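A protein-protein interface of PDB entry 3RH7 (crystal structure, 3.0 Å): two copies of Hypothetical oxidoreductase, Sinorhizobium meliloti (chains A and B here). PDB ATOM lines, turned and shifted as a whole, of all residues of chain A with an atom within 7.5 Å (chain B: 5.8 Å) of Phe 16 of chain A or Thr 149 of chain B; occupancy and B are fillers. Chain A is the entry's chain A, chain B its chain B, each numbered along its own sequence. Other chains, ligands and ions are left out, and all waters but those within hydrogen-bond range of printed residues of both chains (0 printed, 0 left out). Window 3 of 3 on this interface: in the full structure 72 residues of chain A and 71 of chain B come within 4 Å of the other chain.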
ATOM      1  N   ALA A  13      25.126 -10.127 -23.757  1.00  0.00           N
ATOM      2  CA  ALA A  13      24.548 -11.249 -24.492  1.00  0.00           C
ATOM      3  C   ALA A  13      24.776 -12.499 -23.741  1.00  0.00           C
ATOM      4  O   ALA A  13      25.884 -12.717 -23.255  1.00  0.00           O
ATOM      5  CB  ALA A  13      25.177 -11.354 -25.852  1.00  0.00           C
ATOM      6  N   GLU A  14      23.736 -13.325 -23.604  1.00  0.00           N
ATOM      7  CA  GLU A  14      23.763 -14.534 -22.776  1.00  0.00           C
ATOM      8  C   GLU A  14      24.765 -15.571 -23.260  1.00  0.00           C
ATOM      9  O   GLU A  14      24.756 -15.961 -24.426  1.00  0.00           O
ATOM     10  CB  GLU A  14      22.369 -15.155 -22.681  1.00  0.00           C
ATOM     11  CG  GLU A  14      22.251 -16.223 -21.623  1.00  0.00           C
ATOM     12  CD  GLU A  14      20.841 -16.728 -21.423  1.00  0.00           C
ATOM     13  OE1 GLU A  14      20.088 -16.086 -20.649  1.00  0.00           O
ATOM     14  OE2 GLU A  14      20.504 -17.785 -22.007  1.00  0.00           O
ATOM     15  N   VAL A  15      25.614 -16.025 -22.346  1.00  0.00           N
ATOM     16  CA  VAL A  15      26.612 -17.015 -22.704  1.00  0.00           C
ATOM     17  C   VAL A  15      26.193 -18.407 -22.168  1.00  0.00           C
ATOM     18  O   VAL A  15      26.224 -19.375 -22.926  1.00  0.00           O
ATOM     19  CB  VAL A  15      28.027 -16.593 -22.248  1.00  0.00           C
ATOM     20  CG1 VAL A  15      29.040 -17.657 -22.631  1.00  0.00           C
ATOM     21  CG2 VAL A  15      28.425 -15.248 -22.878  1.00  0.00           C
ATOM     22  N   PHE A  16      25.819 -18.502 -20.875  1.00  0.00           N
ATOM     23  CA  PHE A  16      25.374 -19.762 -20.241  1.00  0.00           C
ATOM     24  C   PHE A  16      23.887 -19.680 -19.910  1.00  0.00           C
ATOM     25  O   PHE A  16      23.417 -18.580 -19.585  1.00  0.00           O
ATOM     26  CB  PHE A  16      26.140 -20.041 -18.914  1.00  0.00           C
ATOM     27  CG  PHE A  16      27.633 -20.187 -18.908  1.00  0.00           C
ATOM     28  CD1 PHE A  16      28.267 -20.962 -19.857  1.00  0.00           C
ATOM     29  CD2 PHE A  16      28.404 -19.585 -17.918  1.00  0.00           C
ATOM     30  CE1 PHE A  16      29.656 -21.101 -19.852  1.00  0.00           C
ATOM     31  CE2 PHE A  16      29.786 -19.738 -17.898  1.00  0.00           C
ATOM     32  CZ  PHE A  16      30.407 -20.496 -18.867  1.00  0.00           C
ATOM     33  N   ASP A  17      23.167 -20.835 -19.846  1.00  0.00           N
ATOM     34  CA  ASP A  17      21.753 -20.819 -19.446  1.00  0.00           C
ATOM     35  C   ASP A  17      21.673 -20.569 -17.955  1.00  0.00           C
ATOM     36  O   ASP A  17      22.228 -21.368 -17.185  1.00  0.00           O
ATOM     37  CB  ASP A  17      21.010 -22.118 -19.835  1.00  0.00           C
ATOM     38  CG  ASP A  17      19.600 -22.292 -19.256  1.00  0.00           C
ATOM     39  OD1 ASP A  17      18.898 -21.273 -19.051  1.00  0.00           O
ATOM     40  OD2 ASP A  17      19.195 -23.442 -19.024  1.00  0.00           O
ATOM     41  N   PRO A  18      21.018 -19.467 -17.514  1.00  0.00           N
ATOM     42  CA  PRO A  18      20.919 -19.190 -16.069  1.00  0.00           C
ATOM     43  C   PRO A  18      20.391 -20.387 -15.245  1.00  0.00           C
ATOM     44  O   PRO A  18      20.942 -20.649 -14.174  1.00  0.00           O
ATOM     45  CB  PRO A  18      19.977 -17.990 -16.000  1.00  0.00           C
ATOM     46  CG  PRO A  18      19.327 -17.939 -17.333  1.00  0.00           C
ATOM     47  CD  PRO A  18      20.344 -18.415 -18.281  1.00  0.00           C
ATOM     48  N   ARG A  19      19.394 -21.155 -15.767  1.00  0.00           N
ATOM     49  CA  ARG A  19      18.874 -22.336 -15.066  1.00  0.00           C
ATOM     50  C   ARG A  19      19.973 -23.375 -14.904  1.00  0.00           C
ATOM     51  O   ARG A  19      20.228 -23.789 -13.776  1.00  0.00           O
ATOM     52  CB  ARG A  19      17.653 -22.956 -15.773  1.00  0.00           C
ATOM     53  CG  ARG A  19      17.246 -24.342 -15.204  1.00  0.00           C
ATOM     54  CD  ARG A  19      15.926 -24.869 -15.733  1.00  0.00           C
ATOM     55  NE  ARG A  19      14.786 -23.990 -15.422  1.00  0.00           N
ATOM     56  CZ  ARG A  19      14.169 -23.910 -14.236  1.00  0.00           C
ATOM     57  NH1 ARG A  19      14.595 -24.640 -13.201  1.00  0.00           N
ATOM     58  NH2 ARG A  19      13.140 -23.082 -14.070  1.00  0.00           N
ATOM     59  N   ALA A  20      20.626 -23.765 -16.020  1.00  0.00           N
ATOM     60  CA  ALA A  20      21.693 -24.756 -16.062  1.00  0.00           C
ATOM     61  C   ALA A  20      22.795 -24.429 -15.051  1.00  0.00           C
ATOM     62  O   ALA A  20      23.164 -25.295 -14.237  1.00  0.00           O
ATOM     63  CB  ALA A  20      22.263 -24.836 -17.465  1.00  0.00           C
ATOM     64  N   LEU A  21      23.257 -23.155 -15.063  1.00  0.00           N
ATOM     65  CA  LEU A  21      24.293 -22.677 -14.148  1.00  0.00           C
ATOM     66  C   LEU A  21      23.801 -22.715 -12.705  1.00  0.00           C
ATOM     67  O   LEU A  21      24.514 -23.243 -11.861  1.00  0.00           O
ATOM     68  CB  LEU A  21      24.775 -21.266 -14.518  1.00  0.00           C
ATOM     69  CG  LEU A  21      25.915 -20.711 -13.683  1.00  0.00           C
ATOM     70  CD1 LEU A  21      27.123 -21.610 -13.738  1.00  0.00           C
ATOM     71  CD2 LEU A  21      26.250 -19.302 -14.084  1.00  0.00           C
ATOM     72  N   PRO B  60      29.065 -15.078 -14.420  1.00  0.00           N
ATOM     73  CA  PRO B  60      29.183 -16.276 -13.572  1.00  0.00           C
ATOM     74  C   PRO B  60      30.408 -16.185 -12.634  1.00  0.00           C
ATOM     75  O   PRO B  60      31.556 -16.288 -13.066  1.00  0.00           O
ATOM     76  CB  PRO B  60      29.289 -17.413 -14.587  1.00  0.00           C
ATOM     77  CG  PRO B  60      29.836 -16.800 -15.805  1.00  0.00           C
ATOM     78  CD  PRO B  60      29.347 -15.390 -15.839  1.00  0.00           C
ATOM     79  N   ARG B  81      44.361 -19.724 -14.083  1.00  0.00           N
ATOM     80  CA  ARG B  81      43.157 -20.517 -14.248  1.00  0.00           C
ATOM     81  C   ARG B  81      43.090 -21.622 -13.204  1.00  0.00           C
ATOM     82  O   ARG B  81      44.122 -22.152 -12.780  1.00  0.00           O
ATOM     83  CB  ARG B  81      43.117 -21.106 -15.666  1.00  0.00           C
ATOM     84  CG  ARG B  81      42.982 -20.029 -16.725  1.00  0.00           C
ATOM     85  CD  ARG B  81      42.940 -20.566 -18.143  1.00  0.00           C
ATOM     86  NE  ARG B  81      42.421 -19.564 -19.084  1.00  0.00           N
ATOM     87  CZ  ARG B  81      41.127 -19.305 -19.282  1.00  0.00           C
ATOM     88  NH1 ARG B  81      40.194 -19.967 -18.602  1.00  0.00           N
ATOM     89  NH2 ARG B  81      40.757 -18.376 -20.153  1.00  0.00           N
ATOM     90  N   ASP B 116      40.694 -25.385 -20.753  1.00  0.00           N
ATOM     91  CA  ASP B 116      41.628 -24.367 -20.280  1.00  0.00           C
ATOM     92  C   ASP B 116      42.727 -24.976 -19.354  1.00  0.00           C
ATOM     93  O   ASP B 116      43.267 -24.301 -18.475  1.00  0.00           O
ATOM     94  CB  ASP B 116      40.845 -23.234 -19.598  1.00  0.00           C
ATOM     95  CG  ASP B 116      39.710 -22.667 -20.451  1.00  0.00           C
ATOM     96  OD1 ASP B 116      39.983 -21.752 -21.267  1.00  0.00           O
ATOM     97  OD2 ASP B 116      38.546 -23.161 -20.316  1.00  0.00           O
ATOM     98  N   GLU B 129      35.152 -24.725 -14.490  1.00  0.00           N
ATOM     99  CA  GLU B 129      36.412 -24.230 -15.030  1.00  0.00           C
ATOM    100  C   GLU B 129      36.414 -22.714 -14.901  1.00  0.00           C
ATOM    101  O   GLU B 129      35.463 -22.050 -15.359  1.00  0.00           O
ATOM    102  CB  GLU B 129      36.560 -24.644 -16.501  1.00  0.00           C
ATOM    103  CG  GLU B 129      37.103 -26.034 -16.683  1.00  0.00           C
ATOM    104  CD  GLU B 129      38.185 -26.084 -17.730  1.00  0.00           C
ATOM    105  OE1 GLU B 129      37.836 -26.240 -18.925  1.00  0.00           O
ATOM    106  OE2 GLU B 129      39.376 -25.942 -17.355  1.00  0.00           O
ATOM    107  N   CYS B 130      37.443 -22.152 -14.263  1.00  0.00           N
ATOM    108  CA  CYS B 130      37.434 -20.703 -14.105  1.00  0.00           C
ATOM    109  C   CYS B 130      38.740 -20.050 -14.494  1.00  0.00           C
ATOM    110  O   CYS B 130      39.730 -20.697 -14.785  1.00  0.00           O
ATOM    111  CB  CYS B 130      37.049 -20.309 -12.681  1.00  0.00           C
ATOM    112  SG  CYS B 130      35.856 -21.414 -11.894  1.00  0.00           S
ATOM    113  N   SER B 131      38.696 -18.733 -14.471  1.00  0.00           N
ATOM    114  CA  SER B 131      39.756 -17.765 -14.643  1.00  0.00           C
ATOM    115  C   SER B 131      39.810 -16.950 -13.377  1.00  0.00           C
ATOM    116  O   SER B 131      38.751 -16.561 -12.872  1.00  0.00           O
ATOM    117  CB  SER B 131      39.430 -16.867 -15.822  1.00  0.00           C
ATOM    118  OG  SER B 131      38.284 -16.086 -15.516  1.00  0.00           O
ATOM    119  N   ARG B 147      35.830 -16.619 -12.383  1.00  0.00           N
ATOM    120  CA  ARG B 147      34.806 -16.394 -13.394  1.00  0.00           C
ATOM    121  C   ARG B 147      34.613 -17.671 -14.214  1.00  0.00           C
ATOM    122  O   ARG B 147      35.531 -18.086 -14.914  1.00  0.00           O
ATOM    123  CB  ARG B 147      35.212 -15.237 -14.290  1.00  0.00           C
ATOM    124  CG  ARG B 147      34.040 -14.669 -15.038  1.00  0.00           C
ATOM    125  CD  ARG B 147      34.435 -13.860 -16.255  1.00  0.00           C
ATOM    126  NE  ARG B 147      33.250 -13.189 -16.775  1.00  0.00           N
ATOM    127  CZ  ARG B 147      32.335 -13.774 -17.542  1.00  0.00           C
ATOM    128  NH1 ARG B 147      32.504 -15.036 -17.952  1.00  0.00           N
ATOM    129  NH2 ARG B 147      31.258 -13.102 -17.927  1.00  0.00           N
ATOM    130  N   VAL B 148      33.446 -18.298 -14.125  1.00  0.00           N
ATOM    131  CA  VAL B 148      33.176 -19.589 -14.771  1.00  0.00           C
ATOM    132  C   VAL B 148      33.313 -19.477 -16.305  1.00  0.00           C
ATOM    133  O   VAL B 148      32.687 -18.596 -16.911  1.00  0.00           O
ATOM    134  CB  VAL B 148      31.795 -20.163 -14.329  1.00  0.00           C
ATOM    135  CG1 VAL B 148      31.503 -21.500 -14.991  1.00  0.00           C
ATOM    136  CG2 VAL B 148      31.737 -20.320 -12.820  1.00  0.00           C
ATOM    137  N   THR B 149      34.188 -20.337 -16.919  1.00  0.00           N
ATOM    138  CA  THR B 149      34.424 -20.374 -18.396  1.00  0.00           C
ATOM    139  C   THR B 149      33.700 -21.594 -18.993  1.00  0.00           C
ATOM    140  O   THR B 149      33.367 -21.609 -20.174  1.00  0.00           O
ATOM    141  CB  THR B 149      35.938 -20.353 -18.798  1.00  0.00           C
ATOM    142  OG1 THR B 149      36.543 -21.674 -18.851  1.00  0.00           O
ATOM    143  CG2 THR B 149      36.762 -19.403 -17.948  1.00  0.00           C
ATOM    144  N   ALA B 150      33.467 -22.609 -18.156  1.00  0.00           N
ATOM    145  CA  ALA B 150      32.824 -23.854 -18.529  1.00  0.00           C
ATOM    146  C   ALA B 150      32.348 -24.543 -17.270  1.00  0.00           C
ATOM    147  O   ALA B 150      32.827 -24.230 -16.176  1.00  0.00           O
ATOM    148  CB  ALA B 150      33.822 -24.737 -19.278  1.00  0.00           C
ATOM    149  N   PHE B 151      31.424 -25.485 -17.412  1.00  0.00           N
ATOM    150  CA  PHE B 151      30.906 -26.257 -16.274  1.00  0.00           C
ATOM    151  C   PHE B 151      30.098 -27.473 -16.749  1.00  0.00           C
ATOM    152  O   PHE B 151      29.736 -27.576 -17.929  1.00  0.00           O
ATOM    153  CB  PHE B 151      30.051 -25.399 -15.290  1.00  0.00           C
ATOM    154  CG  PHE B 151      28.750 -24.890 -15.848  1.00  0.00           C
ATOM    155  CD1 PHE B 151      28.695 -23.685 -16.531  1.00  0.00           C
ATOM    156  CD2 PHE B 151      27.579 -25.616 -15.684  1.00  0.00           C
ATOM    157  CE1 PHE B 151      27.491 -23.220 -17.061  1.00  0.00           C
ATOM    158  CE2 PHE B 151      26.365 -25.139 -16.180  1.00  0.00           C
ATOM    159  CZ  PHE B 151      26.329 -23.949 -16.877  1.00  0.00           C
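Of chain A, only Phe 16 (3.4 Å) comes within 4 Å of Thr 149 of chain B.
Of the printed residues of chain B, Leu 21 of chain A touches Pro 60 and Phe 151.
Printed residues of chain A within 4 Å of Phe 151 of chain B: Phe 16 (3.6 Å), Ala 20 (3.7 Å) and Leu 21 (3.6 Å).
Printed residues of chain A within 4 Å of Ala 150 of chain B: Phe 16 (3.8 Å).
Arg 81 of chain B touches none of the printed residues of chain A.
Asp 116 of chain B touches none of the printed residues of chain A.
The nearest residue of chain B that does not touch Phe 16 of chain A is Arg 147 of chain B (5.4 Å).
The nearest residue of chain A that does not touch Thr 149 of chain B is Val 15 of chain A (6.4 Å).
The nearest printed residue of chain A that does not touch Ala 150 of chain B is Leu 21 of chain A (6.7 Å).
No position is printed for both chains.
Of the 8 pairs that touch across the chains among the printed residues, none has its exchanged pair printed and touching as well.
The backbone NH (N) of Ala 20 of chain A lies within hydrogen-bond range of the side-chain carboxylate (OD2) of Asp 17 of chain A (3.3 Å).
The backbone NH (N) of Val 148 of chain B is in hydrogen-bond range of the backbone carbonyl oxygen (O) of Pro 60 of chain B (3.0 Å).
OD2 of Asp 116 of chain B is in hydrogen-bond range of OG1 of Thr 149 of chain B (2.9 Å).
The backbone NH (N) of Thr 149 of chain B sits at hydrogen-bond distance from the backbone carbonyl oxygen (O) of Glu 129 of chain B (2.6 Å).
The backbone carbonyl oxygen of Ala 150 of chain B is in hydrogen-bond range of the backbone NH of Glu 129 of chain B (2.9 Å).
Printed residues of chain B that touch a printed residue of chain A: Pro 60, Val 148, Thr 149, Ala 150 and Phe 151.
Hydrophobic or aromatic side chains of chain B within 4 Å of the printed part of chain A: Pro 60, Val 148 and Phe 151.
Printed residues of chain A that touch a printed residue of chain B: Phe 16, Ala 20 and Leu 21.
Hydrophobic or aromatic side chains of chain A that line the printed part of chain B: Phe 16 and Leu 21.
Among the printed residues, merely in contact across the chains: Phe 16 of chain A with Val 148 of chain B (3.3 Å), Phe 16 of chain A with Thr 149 of chain B (3.4 Å), Phe 16 of chain A with Phe 151 of chain B (3.6 Å), Phe 16 of chain A with Pro 60 of chain B (3.6 Å), Leu 21 of chain A with Pro 60 of chain B (3.6 Å), Leu 21 of chain A with Phe 151 of chain B (3.6 Å), Ala 20 of chain A with Phe 151 of chain B (3.7 Å) and Phe 16 of chain A with Ala 150 of chain B (3.8 Å).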
